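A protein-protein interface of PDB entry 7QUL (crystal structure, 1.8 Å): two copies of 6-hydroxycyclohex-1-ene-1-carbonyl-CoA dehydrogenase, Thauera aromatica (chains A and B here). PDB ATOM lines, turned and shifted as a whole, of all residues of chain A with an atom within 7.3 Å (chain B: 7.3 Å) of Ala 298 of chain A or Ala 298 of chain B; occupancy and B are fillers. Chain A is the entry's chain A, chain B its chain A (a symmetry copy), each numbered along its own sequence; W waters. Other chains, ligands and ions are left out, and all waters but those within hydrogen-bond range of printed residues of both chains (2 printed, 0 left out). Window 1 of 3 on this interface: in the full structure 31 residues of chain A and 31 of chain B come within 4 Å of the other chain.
The backbone carbonyl oxygen of Ala 296 of chain B lies within hydrogen-bond range of the backbone NH of Gly 300 of chain A, 2.9 Å away. The backbone NH of Gly 300 of chain B lies within hydrogen-bond range of the backbone carbonyl oxygen of Ala 296 of chain A, at 2.9 Å. The backbone NH (N) of Ala 298 of chain A sits at hydrogen-bond distance from the backbone carbonyl oxygen (O) of Ala 298 of chain B, at 2.9 Å.
O of Leu 274 of chain A is in hydrogen-bond range of N of Leu 299 of chain A (2.8 Å). The backbone NH (N) of Val 276 of chain A lies within hydrogen-bond range of the backbone carbonyl oxygen (O) of Leu 299 of chain A. The backbone NH (N) of Leu 274 of chain B lies within hydrogen-bond range of the backbone carbonyl oxygen (O) of Arg 297 of chain B (2.9 Å). The backbone carbonyl oxygen (O) of Leu 291 of chain B is in hydrogen-bond range of the backbone NH (N) of Ala 296 of chain B (2.8 Å). OG1 of Thr 273 of chain A lies within hydrogen-bond range of NE of Arg 297 of chain A (2.8 Å). The backbone carbonyl oxygen (O) of Arg 297 of chain A sits at hydrogen-bond distance from the backbone NH (N) of Leu 274 of chain A (2.9 Å).
Among the printed residues, pairs that only touch across the chains: Arg 297 of chain A with Ala 298 of chain B (3.2 Å), Ala 298 of chain A with Arg 297 of chain B (3.2 Å), Leu 291 of chain A with Gly 300 of chain B (3.5 Å), Gly 300 of chain A with Leu 291 of chain B (3.5 Å), Leu 299 of chain A with Arg 297 of chain B (3.6 Å), Arg 297 of chain A with Leu 299 of chain B (3.6 Å), Val 276 of chain A with Leu 288 of chain B (3.9 Å), Leu 288 of chain A with Val 276 of chain B (3.9 Å), Ala 296 of chain A with Leu 299 of chain B (3.9 Å) and Leu 299 of chain A with Ala 296 of chain B (3.9 Å).
Of the printed residues of chain B, Ala 298 of chain A touches Arg 297 and Ala 298. Ala 298 of chain B touches two residues of chain A. Printed residues of chain B within 4 Å of Leu 291 of chain A: Gly 300. Of the printed residues of chain A, Leu 291 of chain B touches Gly 300. Leu 268 of chain B touches none of the printed residues of chain A. Thr 273 of chain A touches none of the printed residues of chain B.
Hydrophobic or aromatic side chains of chain B within 4 Å of the printed part of chain A: Val 276, Leu 291 and Leu 299. Printed residues of chain A that touch a printed residue of chain B: Val 276, Leu 288, Leu 291, Ala 296, Arg 297, Ala 298, Leu 299 and Gly 300. Among the printed residues, 13 pairs touch across the chains. Among the printed residues, no Asp or Glu carboxylate lies within 4 Å of a Lys or Arg side-chain nitrogen of the other chain.
Leu 291 of chain A touches Gly 300 of chain B, and with the chains exchanged Gly 300 of chain A touches Leu 291 of chain B. Ala 296 of chain A touches Gly 300 of chain B, and with the chains exchanged Gly 300 of chain A touches Ala 296 of chain B. Arg 297 of chain A touches Leu 299 of chain B, and with the chains exchanged Leu 299 of chain A touches Arg 297 of chain B. Ala 298 of chain B touches its own counterpart, Ala 298 of chain A. Positions printed for both chains: 167, 265, 268, 272, 273, 274, 275, 276, 288, 291, 296, 297, 298, 299 and 300. Of the 13 pairs that touch across the chains among the printed residues, 13 have their exchanged pair printed and touching as well.
Water W1 lies within hydrogen-bond range of NE2 of Gln 167 of chain A (2.6 Å), O of Ala 296 of chain B (3.1 Å) and O of Gly 300 of chain A (3.1 Å). Water W2 lies within hydrogen-bond range of NE2 of Gln 167 of chain B (2.6 Å), O of Ala 296 of chain A (3.1 Å) and O of Gly 300 of chain B (3.1 Å).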
ATOM      1  N   GLN A 167     -15.298  13.869   3.687  1.00  0.00           N
ATOM      2  CA  GLN A 167     -13.884  13.434   3.924  1.00  0.00           C
ATOM      3  C   GLN A 167     -13.103  14.515   4.683  1.00  0.00           C
ATOM      4  O   GLN A 167     -12.162  14.158   5.429  1.00  0.00           O
ATOM      5  CB  GLN A 167     -13.196  13.043   2.607  1.00  0.00           C
ATOM      6  CG  GLN A 167     -11.742  12.625   2.784  1.00  0.00           C
ATOM      7  CD  GLN A 167     -10.874  12.665   1.542  1.00  0.00           C
ATOM      8  OE1 GLN A 167     -11.280  13.075   0.448  1.00  0.00           O
ATOM      9  NE2 GLN A 167      -9.625  12.247   1.730  1.00  0.00           N
ATOM     10  N   TYR A 265      -4.218  27.392  -1.747  1.00  0.00           N
ATOM     11  CA  TYR A 265      -2.968  27.051  -1.003  1.00  0.00           C
ATOM     12  C   TYR A 265      -2.541  28.263  -0.180  1.00  0.00           C
ATOM     13  O   TYR A 265      -2.139  28.127   1.003  1.00  0.00           O
ATOM     14  CB  TYR A 265      -1.821  26.637  -1.921  1.00  0.00           C
ATOM     15  CG  TYR A 265      -0.743  25.868  -1.214  1.00  0.00           C
ATOM     16  CD1 TYR A 265      -0.842  24.497  -1.063  1.00  0.00           C
ATOM     17  CD2 TYR A 265       0.370  26.505  -0.676  1.00  0.00           C
ATOM     18  CE1 TYR A 265       0.118  23.780  -0.367  1.00  0.00           C
ATOM     19  CE2 TYR A 265       1.359  25.791  -0.020  1.00  0.00           C
ATOM     20  CZ  TYR A 265       1.204  24.435   0.187  1.00  0.00           C
ATOM     21  OH  TYR A 265       2.171  23.703   0.821  1.00  0.00           O
ATOM     22  N   LEU A 268      -4.265  28.716   3.466  1.00  0.00           N
ATOM     23  CA  LEU A 268      -3.937  27.757   4.559  1.00  0.00           C
ATOM     24  C   LEU A 268      -3.760  28.564   5.852  1.00  0.00           C
ATOM     25  O   LEU A 268      -3.108  29.634   5.804  1.00  0.00           O
ATOM     26  CB  LEU A 268      -2.660  26.979   4.220  1.00  0.00           C
ATOM     27  CG  LEU A 268      -2.785  25.829   3.221  1.00  0.00           C
ATOM     28  CD1 LEU A 268      -1.429  25.203   2.951  1.00  0.00           C
ATOM     29  CD2 LEU A 268      -3.762  24.766   3.733  1.00  0.00           C
ATOM     30  N   ALA A 272      -5.533  23.703   9.126  1.00  0.00           N
ATOM     31  CA  ALA A 272      -6.509  23.760   8.009  1.00  0.00           C
ATOM     32  C   ALA A 272      -6.441  22.469   7.194  1.00  0.00           C
ATOM     33  O   ALA A 272      -5.442  21.754   7.241  1.00  0.00           O
ATOM     34  CB  ALA A 272      -6.287  24.971   7.124  1.00  0.00           C
ATOM     35  N   THR A 273      -7.527  22.178   6.496  1.00  0.00           N
ATOM     36  CA  THR A 273      -7.650  21.087   5.501  1.00  0.00           C
ATOM     37  C   THR A 273      -7.823  21.736   4.126  1.00  0.00           C
ATOM     38  O   THR A 273      -8.727  22.628   4.008  1.00  0.00           O
ATOM     39  CB  THR A 273      -8.863  20.227   5.858  1.00  0.00           C
ATOM     40  OG1 THR A 273      -8.581  19.576   7.108  1.00  0.00           O
ATOM     41  CG2 THR A 273      -9.210  19.237   4.773  1.00  0.00           C
ATOM     42  N   LEU A 274      -6.978  21.367   3.167  1.00  0.00           N
ATOM     43  CA  LEU A 274      -7.123  21.813   1.767  1.00  0.00           C
ATOM     44  C   LEU A 274      -7.588  20.607   0.972  1.00  0.00           C
ATOM     45  O   LEU A 274      -6.786  19.669   0.781  1.00  0.00           O
ATOM     46  CB  LEU A 274      -5.817  22.369   1.203  1.00  0.00           C
ATOM     47  CG  LEU A 274      -5.792  22.505  -0.319  1.00  0.00           C
ATOM     48  CD1 LEU A 274      -6.870  23.489  -0.782  1.00  0.00           C
ATOM     49  CD2 LEU A 274      -4.412  22.924  -0.778  1.00  0.00           C
ATOM     50  N   ALA A 275      -8.827  20.676   0.499  1.00  0.00           N
ATOM     51  CA  ALA A 275      -9.470  19.630  -0.320  1.00  0.00           C
ATOM     52  C   ALA A 275      -9.269  19.993  -1.791  1.00  0.00           C
ATOM     53  O   ALA A 275      -9.724  21.062  -2.248  1.00  0.00           O
ATOM     54  CB  ALA A 275     -10.927  19.483   0.035  1.00  0.00           C
ATOM     55  N   VAL A 276      -8.641  19.075  -2.500  1.00  0.00           N
ATOM     56  CA  VAL A 276      -8.355  19.176  -3.951  1.00  0.00           C
ATOM     57  C   VAL A 276      -9.446  18.398  -4.682  1.00  0.00           C
ATOM     58  O   VAL A 276      -9.484  17.146  -4.621  1.00  0.00           O
ATOM     59  CB  VAL A 276      -6.929  18.686  -4.244  1.00  0.00           C
ATOM     60  CG1 VAL A 276      -6.522  18.952  -5.694  1.00  0.00           C
ATOM     61  CG2 VAL A 276      -5.936  19.294  -3.271  1.00  0.00           C
ATOM     62  N   LEU A 288       5.687  23.327  -0.312  1.00  0.00           N
ATOM     63  CA  LEU A 288       5.088  22.162   0.379  1.00  0.00           C
ATOM     64  C   LEU A 288       5.220  22.351   1.897  1.00  0.00           C
ATOM     65  O   LEU A 288       4.349  21.849   2.611  1.00  0.00           O
ATOM     66  CB  LEU A 288       5.775  20.887  -0.121  1.00  0.00           C
ATOM     67  N   LEU A 291       2.532  23.421   4.680  1.00  0.00           N
ATOM     68  CA  LEU A 291       1.742  22.326   5.318  1.00  0.00           C
ATOM     69  C   LEU A 291       2.292  22.065   6.722  1.00  0.00           C
ATOM     70  O   LEU A 291       1.505  21.795   7.647  1.00  0.00           O
ATOM     71  CB  LEU A 291       1.826  21.060   4.453  1.00  0.00           C
ATOM     72  CG  LEU A 291       0.631  20.739   3.544  1.00  0.00           C
ATOM     73  CD1 LEU A 291      -0.207  21.947   3.160  1.00  0.00           C
ATOM     74  CD2 LEU A 291       1.084  20.003   2.297  1.00  0.00           C
ATOM     75  N   ALA A 296      -1.018  21.311   8.632  1.00  0.00           N
ATOM     76  CA  ALA A 296      -2.161  21.237   7.695  1.00  0.00           C
ATOM     77  C   ALA A 296      -2.053  19.971   6.850  1.00  0.00           C
ATOM     78  O   ALA A 296      -0.998  19.313   6.811  1.00  0.00           O
ATOM     79  CB  ALA A 296      -2.205  22.459   6.808  1.00  0.00           C
ATOM     80  N   ARG A 297      -3.128  19.656   6.157  1.00  0.00           N
ATOM     81  CA  ARG A 297      -3.198  18.452   5.310  1.00  0.00           C
ATOM     82  C   ARG A 297      -3.889  18.835   4.009  1.00  0.00           C
ATOM     83  O   ARG A 297      -4.770  19.707   4.056  1.00  0.00           O
ATOM     84  CB  ARG A 297      -3.981  17.337   5.990  1.00  0.00           C
ATOM     85  CG  ARG A 297      -5.349  17.776   6.465  1.00  0.00           C
ATOM     86  CD  ARG A 297      -6.040  16.661   7.237  1.00  0.00           C
ATOM     87  NE  ARG A 297      -7.406  17.107   7.417  1.00  0.00           N
ATOM     88  CZ  ARG A 297      -8.460  16.337   7.675  1.00  0.00           C
ATOM     89  NH1 ARG A 297      -8.329  15.028   7.766  1.00  0.00           N
ATOM     90  NH2 ARG A 297      -9.654  16.892   7.812  1.00  0.00           N
ATOM     91  N   ALA A 298      -3.492  18.169   2.929  1.00  0.00           N
ATOM     92  CA  ALA A 298      -4.080  18.326   1.587  1.00  0.00           C
ATOM     93  C   ALA A 298      -4.709  16.985   1.225  1.00  0.00           C
ATOM     94  O   ALA A 298      -3.986  16.005   1.252  1.00  0.00           O
ATOM     95  CB  ALA A 298      -3.026  18.758   0.593  1.00  0.00           C
ATOM     96  N   LEU A 299      -6.022  16.957   0.993  1.00  0.00           N
ATOM     97  CA  LEU A 299      -6.806  15.724   0.729  1.00  0.00           C
ATOM     98  C   LEU A 299      -7.267  15.713  -0.727  1.00  0.00           C
ATOM     99  O   LEU A 299      -8.185  16.516  -1.050  1.00  0.00           O
ATOM    100  CB  LEU A 299      -8.035  15.694   1.643  1.00  0.00           C
ATOM    101  CG  LEU A 299      -7.736  15.594   3.129  1.00  0.00           C
ATOM    102  CD1 LEU A 299      -9.035  15.409   3.911  1.00  0.00           C
ATOM    103  CD2 LEU A 299      -6.772  14.449   3.388  1.00  0.00           C
ATOM    104  N   GLY A 300      -6.781  14.753  -1.517  1.00  0.00           N
ATOM    105  CA  GLY A 300      -7.228  14.558  -2.907  1.00  0.00           C
ATOM    106  C   GLY A 300      -8.539  13.794  -2.977  1.00  0.00           C
ATOM    107  O   GLY A 300      -8.591  12.669  -2.482  1.00  0.00           O
ATOM    108  N   GLN B 167       1.305   9.824  13.001  1.00  0.00           N
ATOM    109  CA  GLN B 167       0.233  10.605  12.306  1.00  0.00           C
ATOM    110  C   GLN B 167      -0.099   9.979  10.945  1.00  0.00           C
ATOM    111  O   GLN B 167      -1.261  10.112  10.495  1.00  0.00           O
ATOM    112  CB  GLN B 167       0.622  12.086  12.179  1.00  0.00           C
ATOM    113  CG  GLN B 167      -0.419  12.925  11.446  1.00  0.00           C
ATOM    114  CD  GLN B 167       0.059  14.247  10.882  1.00  0.00           C
ATOM    115  OE1 GLN B 167       1.237  14.620  10.939  1.00  0.00           O
ATOM    116  NE2 GLN B 167      -0.891  14.969  10.292  1.00  0.00           N
ATOM    117  N   TYR B 265       6.981  13.282  -4.056  1.00  0.00           N
ATOM    118  CA  TYR B 265       5.682  13.573  -4.734  1.00  0.00           C
ATOM    119  C   TYR B 265       5.543  12.652  -5.943  1.00  0.00           C
ATOM    120  O   TYR B 265       4.449  12.087  -6.198  1.00  0.00           O
ATOM    121  CB  TYR B 265       5.559  15.024  -5.190  1.00  0.00           C
ATOM    122  CG  TYR B 265       4.141  15.449  -5.442  1.00  0.00           C
ATOM    123  CD1 TYR B 265       3.357  15.924  -4.407  1.00  0.00           C
ATOM    124  CD2 TYR B 265       3.570  15.360  -6.706  1.00  0.00           C
ATOM    125  CE1 TYR B 265       2.031  16.271  -4.612  1.00  0.00           C
ATOM    126  CE2 TYR B 265       2.260  15.749  -6.931  1.00  0.00           C
ATOM    127  CZ  TYR B 265       1.470  16.148  -5.871  1.00  0.00           C
ATOM    128  OH  TYR B 265       0.177  16.549  -6.066  1.00  0.00           O
ATOM    129  N   LEU B 268       4.050   8.939  -5.271  1.00  0.00           N
ATOM    130  CA  LEU B 268       2.619   8.781  -4.884  1.00  0.00           C
ATOM    131  C   LEU B 268       2.055   7.582  -5.658  1.00  0.00           C
ATOM    132  O   LEU B 268       2.344   7.465  -6.872  1.00  0.00           O
ATOM    133  CB  LEU B 268       1.835  10.058  -5.206  1.00  0.00           C
ATOM    134  CG  LEU B 268       1.986  11.235  -4.243  1.00  0.00           C
ATOM    135  CD1 LEU B 268       1.197  12.434  -4.733  1.00  0.00           C
ATOM    136  CD2 LEU B 268       1.531  10.846  -2.832  1.00  0.00           C
ATOM    137  N   ALA B 272      -1.967   6.570  -1.152  1.00  0.00           N
ATOM    138  CA  ALA B 272      -0.687   6.820  -0.443  1.00  0.00           C
ATOM    139  C   ALA B 272      -0.832   8.033   0.474  1.00  0.00           C
ATOM    140  O   ALA B 272      -1.720   8.861   0.280  1.00  0.00           O
ATOM    141  CB  ALA B 272       0.469   7.005  -1.407  1.00  0.00           C
ATOM    142  N   THR B 273       0.022   8.089   1.484  1.00  0.00           N
ATOM    143  CA  THR B 273       0.201   9.237   2.404  1.00  0.00           C
ATOM    144  C   THR B 273       1.591   9.822   2.145  1.00  0.00           C
ATOM    145  O   THR B 273       2.578   9.014   2.152  1.00  0.00           O
ATOM    146  CB  THR B 273       0.075   8.740   3.844  1.00  0.00           C
ATOM    147  OG1 THR B 273      -1.281   8.303   4.036  1.00  0.00           O
ATOM    148  CG2 THR B 273       0.477   9.786   4.855  1.00  0.00           C
ATOM    149  N   LEU B 274       1.665  11.122   1.870  1.00  0.00           N
ATOM    150  CA  LEU B 274       2.952  11.833   1.738  1.00  0.00           C
ATOM    151  C   LEU B 274       3.093  12.711   2.968  1.00  0.00           C
ATOM    152  O   LEU B 274       2.347  13.706   3.083  1.00  0.00           O
ATOM    153  CB  LEU B 274       3.018  12.668   0.461  1.00  0.00           C
ATOM    154  CG  LEU B 274       4.145  13.699   0.436  1.00  0.00           C
ATOM    155  CD1 LEU B 274       5.505  13.001   0.519  1.00  0.00           C
ATOM    156  CD2 LEU B 274       4.030  14.562  -0.803  1.00  0.00           C
ATOM    157  N   ALA B 275       4.053  12.359   3.815  1.00  0.00           N
ATOM    158  CA  ALA B 275       4.380  13.085   5.058  1.00  0.00           C
ATOM    159  C   ALA B 275       5.508  14.069   4.745  1.00  0.00           C
ATOM    160  O   ALA B 275       6.612  13.658   4.332  1.00  0.00           O
ATOM    161  CB  ALA B 275       4.750  12.130   6.163  1.00  0.00           C
ATOM    162  N   VAL B 276       5.219  15.331   4.999  1.00  0.00           N
ATOM    163  CA  VAL B 276       6.154  16.467   4.812  1.00  0.00           C
ATOM    164  C   VAL B 276       6.775  16.769   6.173  1.00  0.00           C
ATOM    165  O   VAL B 276       6.088  17.286   7.086  1.00  0.00           O
ATOM    166  CB  VAL B 276       5.419  17.657   4.178  1.00  0.00           C
ATOM    167  CG1 VAL B 276       6.382  18.779   3.788  1.00  0.00           C
ATOM    168  CG2 VAL B 276       4.584  17.209   2.991  1.00  0.00           C
ATOM    169  N   LEU B 288      -0.907  19.390  -8.197  1.00  0.00           N
ATOM    170  CA  LEU B 288      -1.723  19.122  -6.990  1.00  0.00           C
ATOM    171  C   LEU B 288      -2.750  18.025  -7.306  1.00  0.00           C
ATOM    172  O   LEU B 288      -3.101  17.290  -6.381  1.00  0.00           O
ATOM    173  CB  LEU B 288      -2.375  20.432  -6.536  1.00  0.00           C
ATOM    174  N   LEU B 291      -2.851  14.129  -6.346  1.00  0.00           N
ATOM    175  CA  LEU B 291      -3.501  13.765  -5.051  1.00  0.00           C
ATOM    176  C   LEU B 291      -4.886  13.180  -5.334  1.00  0.00           C
ATOM    177  O   LEU B 291      -5.302  12.230  -4.645  1.00  0.00           O
ATOM    178  CB  LEU B 291      -3.605  15.011  -4.160  1.00  0.00           C
ATOM    179  CG  LEU B 291      -2.566  15.172  -3.040  1.00  0.00           C
ATOM    180  CD1 LEU B 291      -1.257  14.443  -3.288  1.00  0.00           C
ATOM    181  CD2 LEU B 291      -2.298  16.640  -2.761  1.00  0.00           C
ATOM    182  N   ALA B 296      -5.043  10.420  -2.590  1.00  0.00           N
ATOM    183  CA  ALA B 296      -3.879  10.514  -1.681  1.00  0.00           C
ATOM    184  C   ALA B 296      -4.009  11.759  -0.807  1.00  0.00           C
ATOM    185  O   ALA B 296      -4.834  12.650  -1.077  1.00  0.00           O
ATOM    186  CB  ALA B 296      -2.590  10.555  -2.466  1.00  0.00           C
ATOM    187  N   ARG B 297      -3.176  11.829   0.211  1.00  0.00           N
ATOM    188  CA  ARG B 297      -3.186  12.952   1.165  1.00  0.00           C
ATOM    189  C   ARG B 297      -1.742  13.332   1.455  1.00  0.00           C
ATOM    190  O   ARG B 297      -0.892  12.428   1.451  1.00  0.00           O
ATOM    191  CB  ARG B 297      -3.879  12.570   2.467  1.00  0.00           C
ATOM    192  CG  ARG B 297      -3.326  11.305   3.087  1.00  0.00           C
ATOM    193  CD  ARG B 297      -4.128  10.907   4.318  1.00  0.00           C
ATOM    194  NE  ARG B 297      -3.366   9.849   4.948  1.00  0.00           N
ATOM    195  CZ  ARG B 297      -3.451   9.466   6.219  1.00  0.00           C
ATOM    196  NH1 ARG B 297      -4.270  10.077   7.052  1.00  0.00           N
ATOM    197  NH2 ARG B 297      -2.683   8.479   6.653  1.00  0.00           N
ATOM    198  N   ALA B 298      -1.526  14.618   1.713  1.00  0.00           N
ATOM    199  CA  ALA B 298      -0.221  15.188   2.092  1.00  0.00           C
ATOM    200  C   ALA B 298      -0.377  15.734   3.507  1.00  0.00           C
ATOM    201  O   ALA B 298      -1.261  16.552   3.696  1.00  0.00           O
ATOM    202  CB  ALA B 298       0.201  16.252   1.106  1.00  0.00           C
ATOM    203  N   LEU B 299       0.398  15.217   4.462  1.00  0.00           N
ATOM    204  CA  LEU B 299       0.305  15.561   5.903  1.00  0.00           C
ATOM    205  C   LEU B 299       1.540  16.357   6.320  1.00  0.00           C
ATOM    206  O   LEU B 299       2.631  15.728   6.413  1.00  0.00           O
ATOM    207  CB  LEU B 299       0.235  14.275   6.733  1.00  0.00           C
ATOM    208  CG  LEU B 299      -1.003  13.423   6.507  1.00  0.00           C
ATOM    209  CD1 LEU B 299      -1.028  12.266   7.503  1.00  0.00           C
ATOM    210  CD2 LEU B 299      -2.250  14.280   6.629  1.00  0.00           C
ATOM    211  N   GLY B 300       1.354  17.621   6.708  1.00  0.00           N
ATOM    212  CA  GLY B 300       2.439  18.462   7.242  1.00  0.00           C
ATOM    213  C   GLY B 300       2.710  18.172   8.708  1.00  0.00           C
ATOM    214  O   GLY B 300       1.792  18.313   9.515  1.00  0.00           O
HETATM  215  O   HOH W   1      -7.453  11.920   0.327  1.00  0.00           O
HETATM  216  O   HOH W   2      -1.118  17.267   9.084  1.00  0.00           O
